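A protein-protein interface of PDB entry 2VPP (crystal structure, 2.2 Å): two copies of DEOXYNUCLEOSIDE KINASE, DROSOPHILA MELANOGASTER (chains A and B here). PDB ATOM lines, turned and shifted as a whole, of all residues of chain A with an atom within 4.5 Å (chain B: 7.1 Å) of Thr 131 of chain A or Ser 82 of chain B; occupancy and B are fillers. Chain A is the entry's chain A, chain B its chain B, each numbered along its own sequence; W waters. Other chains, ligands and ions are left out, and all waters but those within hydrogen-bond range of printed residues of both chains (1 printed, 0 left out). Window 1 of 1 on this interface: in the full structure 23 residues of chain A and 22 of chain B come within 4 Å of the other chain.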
ATOM      1  N   MET A  78     -32.509 -22.030  19.196  1.00  0.00           N
ATOM      2  CA  MET A  78     -31.104 -22.470  19.051  1.00  0.00           C
ATOM      3  C   MET A  78     -30.458 -22.101  17.714  1.00  0.00           C
ATOM      4  O   MET A  78     -29.392 -21.514  17.729  1.00  0.00           O
ATOM      5  CB  MET A  78     -30.894 -23.970  19.392  1.00  0.00           C
ATOM      6  CG  MET A  78     -29.391 -24.374  19.716  1.00  0.00           C
ATOM      7  SD  MET A  78     -28.434 -24.693  18.218  1.00  0.00           S
ATOM      8  CE  MET A  78     -26.737 -24.450  18.747  1.00  0.00           C
ATOM      9  N   GLY A 127     -28.804 -29.234  26.453  1.00  0.00           N
ATOM     10  CA  GLY A 127     -27.847 -29.556  25.386  1.00  0.00           C
ATOM     11  C   GLY A 127     -27.715 -28.448  24.349  1.00  0.00           C
ATOM     12  O   GLY A 127     -26.626 -28.234  23.803  1.00  0.00           O
ATOM     13  N   MET A 128     -28.826 -27.748  24.086  1.00  0.00           N
ATOM     14  CA  MET A 128     -28.872 -26.612  23.141  1.00  0.00           C
ATOM     15  C   MET A 128     -28.139 -25.396  23.688  1.00  0.00           C
ATOM     16  O   MET A 128     -27.310 -24.790  23.014  1.00  0.00           O
ATOM     17  CB  MET A 128     -30.313 -26.238  22.848  1.00  0.00           C
ATOM     18  CG  MET A 128     -30.993 -27.174  21.872  1.00  0.00           C
ATOM     19  SD  MET A 128     -32.749 -26.928  22.049  1.00  0.00           S
ATOM     20  CE  MET A 128     -33.377 -28.471  21.327  1.00  0.00           C
ATOM     21  N   TYR A 129     -28.470 -25.058  24.929  1.00  0.00           N
ATOM     22  CA  TYR A 129     -27.768 -24.059  25.692  1.00  0.00           C
ATOM     23  C   TYR A 129     -26.269 -24.399  25.789  1.00  0.00           C
ATOM     24  O   TYR A 129     -25.419 -23.551  25.488  1.00  0.00           O
ATOM     25  CB  TYR A 129     -28.428 -23.934  27.078  1.00  0.00           C
ATOM     26  CG  TYR A 129     -27.654 -23.061  28.040  1.00  0.00           C
ATOM     27  CD1 TYR A 129     -27.724 -21.660  27.951  1.00  0.00           C
ATOM     28  CD2 TYR A 129     -26.830 -23.634  29.028  1.00  0.00           C
ATOM     29  CE1 TYR A 129     -27.005 -20.843  28.825  1.00  0.00           C
ATOM     30  CE2 TYR A 129     -26.108 -22.831  29.910  1.00  0.00           C
ATOM     31  CZ  TYR A 129     -26.204 -21.433  29.795  1.00  0.00           C
ATOM     32  OH  TYR A 129     -25.512 -20.628  30.656  1.00  0.00           O
ATOM     33  N   ASN A 130     -25.939 -25.630  26.186  1.00  0.00           N
ATOM     34  CA  ASN A 130     -24.531 -26.068  26.267  1.00  0.00           C
ATOM     35  C   ASN A 130     -23.744 -25.932  24.958  1.00  0.00           C
ATOM     36  O   ASN A 130     -22.550 -25.597  24.982  1.00  0.00           O
ATOM     37  CB  ASN A 130     -24.399 -27.515  26.770  1.00  0.00           C
ATOM     38  CG  ASN A 130     -24.803 -27.685  28.221  1.00  0.00           C
ATOM     39  OD1 ASN A 130     -25.127 -26.715  28.923  1.00  0.00           O
ATOM     40  ND2 ASN A 130     -24.790 -28.940  28.686  1.00  0.00           N
ATOM     41  N   THR A 131     -24.388 -26.207  23.820  1.00  0.00           N
ATOM     42  CA  THR A 131     -23.724 -26.025  22.500  1.00  0.00           C
ATOM     43  C   THR A 131     -23.403 -24.554  22.237  1.00  0.00           C
ATOM     44  O   THR A 131     -22.319 -24.227  21.778  1.00  0.00           O
ATOM     45  CB  THR A 131     -24.566 -26.574  21.313  1.00  0.00           C
ATOM     46  OG1 THR A 131     -24.911 -27.936  21.559  1.00  0.00           O
ATOM     47  CG2 THR A 131     -23.796 -26.469  19.986  1.00  0.00           C
ATOM     48  N   LEU A 132     -24.348 -23.669  22.518  1.00  0.00           N
ATOM     49  CA  LEU A 132     -24.127 -22.231  22.293  1.00  0.00           C
ATOM     50  C   LEU A 132     -22.992 -21.691  23.184  1.00  0.00           C
ATOM     51  O   LEU A 132     -22.185 -20.868  22.727  1.00  0.00           O
ATOM     52  CB  LEU A 132     -25.421 -21.417  22.494  1.00  0.00           C
ATOM     53  CG  LEU A 132     -26.603 -21.632  21.542  1.00  0.00           C
ATOM     54  CD1 LEU A 132     -27.921 -21.159  22.160  1.00  0.00           C
ATOM     55  CD2 LEU A 132     -26.360 -20.953  20.217  1.00  0.00           C
ATOM     56  N   GLU A 133     -22.940 -22.171  24.428  1.00  0.00           N
ATOM     57  CA  GLU A 133     -21.903 -21.821  25.397  1.00  0.00           C
ATOM     58  C   GLU A 133     -20.506 -22.289  25.004  1.00  0.00           C
ATOM     59  O   GLU A 133     -19.528 -21.544  25.200  1.00  0.00           O
ATOM     60  CB  GLU A 133     -22.274 -22.354  26.779  1.00  0.00           C
ATOM     61  CG  GLU A 133     -23.208 -21.421  27.578  1.00  0.00           C
ATOM     62  CD  GLU A 133     -22.480 -20.176  28.073  1.00  0.00           C
ATOM     63  OE1 GLU A 133     -21.493 -20.321  28.836  1.00  0.00           O
ATOM     64  OE2 GLU A 133     -22.866 -19.057  27.674  1.00  0.00           O
ATOM     65  N   GLU A 134     -20.415 -23.493  24.418  1.00  0.00           N
ATOM     66  CA  GLU A 134     -19.152 -23.985  23.853  1.00  0.00           C
ATOM     67  C   GLU A 134     -18.659 -23.105  22.710  1.00  0.00           C
ATOM     68  O   GLU A 134     -17.457 -22.822  22.612  1.00  0.00           O
ATOM     69  CB  GLU A 134     -19.254 -25.453  23.413  1.00  0.00           C
ATOM     70  CG  GLU A 134     -19.558 -26.419  24.537  1.00  0.00           C
ATOM     71  CD  GLU A 134     -18.394 -26.650  25.530  1.00  0.00           C
ATOM     72  OE1 GLU A 134     -18.654 -27.319  26.560  1.00  0.00           O
ATOM     73  OE2 GLU A 134     -17.234 -26.200  25.288  1.00  0.00           O
ATOM     74  N   TRP A 135     -19.583 -22.661  21.856  1.00  0.00           N
ATOM     75  CA  TRP A 135     -19.242 -21.658  20.853  1.00  0.00           C
ATOM     76  C   TRP A 135     -18.714 -20.348  21.447  1.00  0.00           C
ATOM     77  O   TRP A 135     -17.675 -19.871  21.015  1.00  0.00           O
ATOM     78  CB  TRP A 135     -20.407 -21.400  19.896  1.00  0.00           C
ATOM     79  CG  TRP A 135     -20.422 -22.370  18.726  1.00  0.00           C
ATOM     80  CD1 TRP A 135     -21.265 -23.441  18.543  1.00  0.00           C
ATOM     81  CD2 TRP A 135     -19.546 -22.354  17.599  1.00  0.00           C
ATOM     82  NE1 TRP A 135     -20.964 -24.089  17.370  1.00  0.00           N
ATOM     83  CE2 TRP A 135     -19.918 -23.442  16.764  1.00  0.00           C
ATOM     84  CE3 TRP A 135     -18.492 -21.511  17.198  1.00  0.00           C
ATOM     85  CZ2 TRP A 135     -19.267 -23.719  15.549  1.00  0.00           C
ATOM     86  CZ3 TRP A 135     -17.834 -21.795  16.002  1.00  0.00           C
ATOM     87  CH2 TRP A 135     -18.229 -22.903  15.188  1.00  0.00           C
ATOM     88  N   VAL B  60     -21.209 -33.232  26.649  1.00  0.00           N
ATOM     89  CA  VAL B  60     -21.192 -31.774  26.586  1.00  0.00           C
ATOM     90  C   VAL B  60     -21.739 -31.270  27.924  1.00  0.00           C
ATOM     91  O   VAL B  60     -22.947 -31.061  28.103  1.00  0.00           O
ATOM     92  CB  VAL B  60     -21.939 -31.193  25.349  1.00  0.00           C
ATOM     93  CG1 VAL B  60     -21.445 -29.790  25.057  1.00  0.00           C
ATOM     94  CG2 VAL B  60     -21.707 -32.055  24.115  1.00  0.00           C
ATOM     95  N   LEU B  65     -24.902 -35.474  23.235  1.00  0.00           N
ATOM     96  CA  LEU B  65     -25.550 -34.939  22.032  1.00  0.00           C
ATOM     97  C   LEU B  65     -25.672 -35.979  20.930  1.00  0.00           C
ATOM     98  O   LEU B  65     -26.618 -35.936  20.111  1.00  0.00           O
ATOM     99  CB  LEU B  65     -24.800 -33.722  21.488  1.00  0.00           C
ATOM    100  CG  LEU B  65     -25.050 -32.345  22.067  1.00  0.00           C
ATOM    101  CD1 LEU B  65     -24.124 -31.351  21.370  1.00  0.00           C
ATOM    102  CD2 LEU B  65     -26.501 -31.968  21.915  1.00  0.00           C
ATOM    103  N   TRP B  76     -32.532 -32.733  17.496  1.00  0.00           N
ATOM    104  CA  TRP B  76     -31.134 -32.621  17.896  1.00  0.00           C
ATOM    105  C   TRP B  76     -30.046 -32.608  16.793  1.00  0.00           C
ATOM    106  O   TRP B  76     -28.882 -32.328  17.085  1.00  0.00           O
ATOM    107  CB  TRP B  76     -30.842 -33.686  18.955  1.00  0.00           C
ATOM    108  CG  TRP B  76     -31.560 -33.419  20.249  1.00  0.00           C
ATOM    109  CD1 TRP B  76     -32.715 -33.992  20.676  1.00  0.00           C
ATOM    110  CD2 TRP B  76     -31.176 -32.480  21.261  1.00  0.00           C
ATOM    111  NE1 TRP B  76     -33.074 -33.484  21.899  1.00  0.00           N
ATOM    112  CE2 TRP B  76     -32.143 -32.552  22.285  1.00  0.00           C
ATOM    113  CE3 TRP B  76     -30.097 -31.601  21.410  1.00  0.00           C
ATOM    114  CZ2 TRP B  76     -32.063 -31.778  23.464  1.00  0.00           C
ATOM    115  CZ3 TRP B  76     -30.012 -30.823  22.578  1.00  0.00           C
ATOM    116  CH2 TRP B  76     -30.996 -30.923  23.589  1.00  0.00           C
ATOM    117  N   ALA B  77     -30.409 -32.884  15.538  1.00  0.00           N
ATOM    118  CA  ALA B  77     -29.430 -32.852  14.418  1.00  0.00           C
ATOM    119  C   ALA B  77     -28.716 -31.509  14.297  1.00  0.00           C
ATOM    120  O   ALA B  77     -27.500 -31.451  14.069  1.00  0.00           O
ATOM    121  CB  ALA B  77     -30.107 -33.194  13.113  1.00  0.00           C
ATOM    122  N   MET B  78     -29.482 -30.430  14.462  1.00  0.00           N
ATOM    123  CA  MET B  78     -28.976 -29.055  14.404  1.00  0.00           C
ATOM    124  C   MET B  78     -27.913 -28.723  15.476  1.00  0.00           C
ATOM    125  O   MET B  78     -26.780 -28.418  15.142  1.00  0.00           O
ATOM    126  CB  MET B  78     -30.168 -28.087  14.448  1.00  0.00           C
ATOM    127  CG  MET B  78     -29.810 -26.635  14.772  1.00  0.00           C
ATOM    128  SD  MET B  78     -28.998 -25.952  13.362  1.00  0.00           S
ATOM    129  CE  MET B  78     -27.911 -24.785  14.212  1.00  0.00           C
ATOM    130  N   PRO B  79     -28.276 -28.764  16.777  1.00  0.00           N
ATOM    131  CA  PRO B  79     -27.223 -28.471  17.760  1.00  0.00           C
ATOM    132  C   PRO B  79     -26.075 -29.491  17.754  1.00  0.00           C
ATOM    133  O   PRO B  79     -24.919 -29.114  17.989  1.00  0.00           O
ATOM    134  CB  PRO B  79     -27.983 -28.443  19.096  1.00  0.00           C
ATOM    135  CG  PRO B  79     -29.181 -29.283  18.869  1.00  0.00           C
ATOM    136  CD  PRO B  79     -29.575 -29.018  17.432  1.00  0.00           C
ATOM    137  N   PHE B  80     -26.360 -30.757  17.448  1.00  0.00           N
ATOM    138  CA  PHE B  80     -25.283 -31.767  17.367  1.00  0.00           C
ATOM    139  C   PHE B  80     -24.250 -31.442  16.290  1.00  0.00           C
ATOM    140  O   PHE B  80     -23.049 -31.418  16.569  1.00  0.00           O
ATOM    141  CB  PHE B  80     -25.842 -33.187  17.164  1.00  0.00           C
ATOM    142  CG  PHE B  80     -24.791 -34.205  16.801  1.00  0.00           C
ATOM    143  CD1 PHE B  80     -23.950 -34.732  17.777  1.00  0.00           C
ATOM    144  CD2 PHE B  80     -24.649 -34.638  15.494  1.00  0.00           C
ATOM    145  CE1 PHE B  80     -22.981 -35.667  17.452  1.00  0.00           C
ATOM    146  CE2 PHE B  80     -23.692 -35.584  15.150  1.00  0.00           C
ATOM    147  CZ  PHE B  80     -22.851 -36.104  16.131  1.00  0.00           C
ATOM    148  N   GLN B  81     -24.721 -31.208  15.061  1.00  0.00           N
ATOM    149  CA  GLN B  81     -23.862 -30.817  13.943  1.00  0.00           C
ATOM    150  C   GLN B  81     -23.137 -29.483  14.150  1.00  0.00           C
ATOM    151  O   GLN B  81     -21.997 -29.333  13.725  1.00  0.00           O
ATOM    152  CB  GLN B  81     -24.645 -30.799  12.614  1.00  0.00           C
ATOM    153  CG  GLN B  81     -25.005 -32.193  12.088  1.00  0.00           C
ATOM    154  CD  GLN B  81     -23.786 -33.097  11.828  1.00  0.00           C
ATOM    155  OE1 GLN B  81     -22.665 -32.624  11.620  1.00  0.00           O
ATOM    156  NE2 GLN B  81     -24.011 -34.397  11.831  1.00  0.00           N
ATOM    157  N   SER B  82     -23.797 -28.518  14.780  1.00  0.00           N
ATOM    158  CA  SER B  82     -23.135 -27.273  15.206  1.00  0.00           C
ATOM    159  C   SER B  82     -21.954 -27.545  16.158  1.00  0.00           C
ATOM    160  O   SER B  82     -20.884 -26.956  16.004  1.00  0.00           O
ATOM    161  CB  SER B  82     -24.147 -26.335  15.874  1.00  0.00           C
ATOM    162  OG  SER B  82     -23.472 -25.275  16.527  1.00  0.00           O
ATOM    163  N   TYR B  83     -22.155 -28.433  17.134  1.00  0.00           N
ATOM    164  CA  TYR B  83     -21.081 -28.848  18.043  1.00  0.00           C
ATOM    165  C   TYR B  83     -20.009 -29.687  17.336  1.00  0.00           C
ATOM    166  O   TYR B  83     -18.815 -29.519  17.606  1.00  0.00           O
ATOM    167  CB  TYR B  83     -21.616 -29.572  19.294  1.00  0.00           C
ATOM    168  CG  TYR B  83     -20.553 -29.775  20.357  1.00  0.00           C
ATOM    169  CD1 TYR B  83     -19.871 -28.675  20.917  1.00  0.00           C
ATOM    170  CD2 TYR B  83     -20.201 -31.063  20.796  1.00  0.00           C
ATOM    171  CE1 TYR B  83     -18.870 -28.850  21.883  1.00  0.00           C
ATOM    172  CE2 TYR B  83     -19.199 -31.255  21.779  1.00  0.00           C
ATOM    173  CZ  TYR B  83     -18.540 -30.140  22.314  1.00  0.00           C
ATOM    174  OH  TYR B  83     -17.556 -30.305  23.269  1.00  0.00           O
ATOM    175  N   VAL B  84     -20.431 -30.578  16.429  1.00  0.00           N
ATOM    176  CA  VAL B  84     -19.483 -31.278  15.541  1.00  0.00           C
ATOM    177  C   VAL B  84     -18.625 -30.286  14.765  1.00  0.00           C
ATOM    178  O   VAL B  84     -17.407 -30.425  14.732  1.00  0.00           O
ATOM    179  CB  VAL B  84     -20.166 -32.282  14.564  1.00  0.00           C
ATOM    180  CG1 VAL B  84     -19.222 -32.651  13.422  1.00  0.00           C
ATOM    181  CG2 VAL B  84     -20.632 -33.541  15.309  1.00  0.00           C
ATOM    182  N   THR B  85     -19.259 -29.281  14.161  1.00  0.00           N
ATOM    183  CA  THR B  85     -18.531 -28.230  13.428  1.00  0.00           C
ATOM    184  C   THR B  85     -17.480 -27.563  14.304  1.00  0.00           C
ATOM    185  O   THR B  85     -16.352 -27.360  13.880  1.00  0.00           O
ATOM    186  CB  THR B  85     -19.504 -27.161  12.872  1.00  0.00           C
ATOM    187  OG1 THR B  85     -20.410 -27.782  11.957  1.00  0.00           O
ATOM    188  CG2 THR B  85     -18.766 -26.041  12.160  1.00  0.00           C
ATOM    189  N   LEU B  86     -17.855 -27.219  15.528  1.00  0.00           N
ATOM    190  CA  LEU B  86     -16.924 -26.589  16.472  1.00  0.00           C
ATOM    191  C   LEU B  86     -15.727 -27.486  16.869  1.00  0.00           C
ATOM    192  O   LEU B  86     -14.586 -27.045  16.820  1.00  0.00           O
ATOM    193  CB  LEU B  86     -17.671 -26.104  17.721  1.00  0.00           C
ATOM    194  CG  LEU B  86     -16.844 -25.502  18.863  1.00  0.00           C
ATOM    195  CD1 LEU B  86     -16.196 -24.211  18.409  1.00  0.00           C
ATOM    196  CD2 LEU B  86     -17.734 -25.260  20.061  1.00  0.00           C
ATOM    197  N   THR B  87     -15.994 -28.720  17.278  1.00  0.00           N
ATOM    198  CA  THR B  87     -14.929 -29.693  17.632  1.00  0.00           C
ATOM    199  C   THR B  87     -13.978 -29.953  16.477  1.00  0.00           C
ATOM    200  O   THR B  87     -12.759 -30.007  16.655  1.00  0.00           O
ATOM    201  CB  THR B  87     -15.513 -31.029  18.090  1.00  0.00           C
ATOM    202  OG1 THR B  87     -16.429 -31.524  17.103  1.00  0.00           O
ATOM    203  CG2 THR B  87     -16.239 -30.862  19.394  1.00  0.00           C
ATOM    204  N   VAL B 115     -24.206 -33.344   7.088  1.00  0.00           N
ATOM    205  CA  VAL B 115     -25.199 -32.276   7.070  1.00  0.00           C
ATOM    206  C   VAL B 115     -26.059 -32.320   5.807  1.00  0.00           C
ATOM    207  O   VAL B 115     -27.293 -32.180   5.887  1.00  0.00           O
ATOM    208  CB  VAL B 115     -24.551 -30.857   7.315  1.00  0.00           C
ATOM    209  CG1 VAL B 115     -25.523 -29.717   6.956  1.00  0.00           C
ATOM    210  CG2 VAL B 115     -24.094 -30.747   8.764  1.00  0.00           C
ATOM    211  N   LEU B 132     -26.263 -23.635   9.559  1.00  0.00           N
ATOM    212  CA  LEU B 132     -25.022 -24.430   9.541  1.00  0.00           C
ATOM    213  C   LEU B 132     -24.128 -24.061   8.346  1.00  0.00           C
ATOM    214  O   LEU B 132     -22.904 -23.991   8.472  1.00  0.00           O
ATOM    215  CB  LEU B 132     -25.324 -25.941   9.541  1.00  0.00           C
ATOM    216  CG  LEU B 132     -26.007 -26.558  10.761  1.00  0.00           C
ATOM    217  CD1 LEU B 132     -26.441 -27.947  10.460  1.00  0.00           C
ATOM    218  CD2 LEU B 132     -25.124 -26.532  12.045  1.00  0.00           C
ATOM    219  N   TRP B 135     -22.202 -20.707   8.956  1.00  0.00           N
ATOM    220  CA  TRP B 135     -21.023 -20.996   9.759  1.00  0.00           C
ATOM    221  C   TRP B 135     -19.873 -21.592   8.928  1.00  0.00           C
ATOM    222  O   TRP B 135     -18.732 -21.135   9.044  1.00  0.00           O
ATOM    223  CB  TRP B 135     -21.394 -21.896  10.930  1.00  0.00           C
ATOM    224  CG  TRP B 135     -21.786 -21.125  12.175  1.00  0.00           C
ATOM    225  CD1 TRP B 135     -23.042 -20.995  12.708  1.00  0.00           C
ATOM    226  CD2 TRP B 135     -20.911 -20.385  13.035  1.00  0.00           C
ATOM    227  NE1 TRP B 135     -23.001 -20.224  13.832  1.00  0.00           N
ATOM    228  CE2 TRP B 135     -21.708 -19.832  14.061  1.00  0.00           C
ATOM    229  CE3 TRP B 135     -19.538 -20.122  13.028  1.00  0.00           C
ATOM    230  CZ2 TRP B 135     -21.169 -19.060  15.098  1.00  0.00           C
ATOM    231  CZ3 TRP B 135     -19.001 -19.329  14.052  1.00  0.00           C
ATOM    232  CH2 TRP B 135     -19.817 -18.815  15.069  1.00  0.00           C
ATOM    233  N   TYR B 136     -20.171 -22.583   8.082  1.00  0.00           N
ATOM    234  CA  TYR B 136     -19.161 -23.192   7.185  1.00  0.00           C
ATOM    235  C   TYR B 136     -18.530 -22.179   6.217  1.00  0.00           C
ATOM    236  O   TYR B 136     -17.311 -22.178   6.017  1.00  0.00           O
ATOM    237  CB  TYR B 136     -19.770 -24.336   6.358  1.00  0.00           C
ATOM    238  CG  TYR B 136     -20.157 -25.593   7.137  1.00  0.00           C
ATOM    239  CD1 TYR B 136     -21.399 -26.200   6.928  1.00  0.00           C
ATOM    240  CD2 TYR B 136     -19.283 -26.174   8.063  1.00  0.00           C
ATOM    241  CE1 TYR B 136     -21.770 -27.333   7.603  1.00  0.00           C
ATOM    242  CE2 TYR B 136     -19.655 -27.332   8.765  1.00  0.00           C
ATOM    243  CZ  TYR B 136     -20.899 -27.897   8.524  1.00  0.00           C
ATOM    244  OH  TYR B 136     -21.283 -29.028   9.187  1.00  0.00           O
HETATM  245  O   HOH W   1     -15.957 -28.235  23.563  1.00  0.00           O
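Trp 135 of chain B touches its own counterpart, Trp 135 of chain A.
Water W1 lies within hydrogen-bond range of OH of Tyr 83 of chain B (2.6 Å) and OE2 of Glu 134 of chain A (3.0 Å).
Printed residues of chain B within 4 Å of Met 78 of chain A: Pro 79.
Thr 131 of chain A touches just these residues of chain B: Leu 65 (3.5 Å), Pro 79 (3.5 Å), Ser 82 (3.7 Å) and Tyr 83 (3.8 Å).
Of the printed residues of chain A, Trp 76 of chain B touches Gly 127 and Met 128.
Of chain A, only Thr 131 and Trp 135 come within 4 Å of Ser 82 of chain B.
Printed residues of chain A within 4 Å of Tyr 83 of chain B: Thr 131 (3.8 Å) and Glu 134 (3.7 Å).
Of the printed residues of chain A, Leu 86 of chain B touches Glu 134 and Trp 135.
Thr 87 of chain B touches none of the printed residues of chain A.
The nearest residue of chain A that does not touch Ser 82 of chain B is Met 78 of chain A (4.03 Å).
The nearest printed residue of chain A that does not touch Pro 79 of chain B is Met 128 of chain A (4.1 Å).
The indole nitrogen of Trp 135 of chain A is in hydrogen-bond range of the side-chain hydroxyl of Ser 82 of chain B (2.9 Å).
The side-chain amide nitrogen (ND2) of Asn 130 of chain A is in hydrogen-bond range of the backbone carbonyl oxygen (O) of Val 60 of chain B, at 2.9 Å.
The side-chain hydroxyl of Thr 87 of chain B sits at hydrogen-bond distance from the backbone carbonyl oxygen of Tyr 83 of chain B, at 3.2 Å.
The backbone carbonyl oxygen of Gly 127 of chain A sits at hydrogen-bond distance from the side-chain hydroxyl of Thr 131 of chain A (2.8 Å).
Hydrophobic or aromatic side chains of chain A within 4 Å of the printed part of chain B: Met 78, Met 128 and Trp 135.
Printed residues of chain B that touch a printed residue of chain A: Val 60, Leu 65, Trp 76, Pro 79, Ser 82, Tyr 83, Leu 86 and Trp 135.
Hydrophobic or aromatic side chains of chain B that line the printed part of chain A: Val 60, Leu 65, Trp 76, Pro 79, Tyr 83, Leu 86 and Trp 135.
Among the printed residues, no Asp or Glu carboxylate lies within 4 Å of a Lys or Arg side-chain nitrogen of the other chain.
Among the printed residues, merely in contact across the chains: Met 78 of chain A with Pro 79 of chain B (3.9 Å), Gly 127 of chain A with Trp 76 of chain B (3.7 Å), Met 128 of chain A with Trp 76 of chain B (3.6 Å), Thr 131 of chain A with Leu 65 of chain B (3.5 Å), Thr 131 of chain A with Pro 79 of chain B (3.5 Å), Thr 131 of chain A with Ser 82 of chain B (3.7 Å), Thr 131 of chain A with Tyr 83 of chain B (3.8 Å), Glu 134 of chain A with Val 60 of chain B (3.9 Å), Glu 134 of chain A with Tyr 83 of chain B (3.7 Å), Glu 134 of chain A with Leu 86 of chain B (3.5 Å), Trp 135 of chain A with Leu 86 of chain B (3.6 Å) and Trp 135 of chain A with Trp 135 of chain B (3.4 Å).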
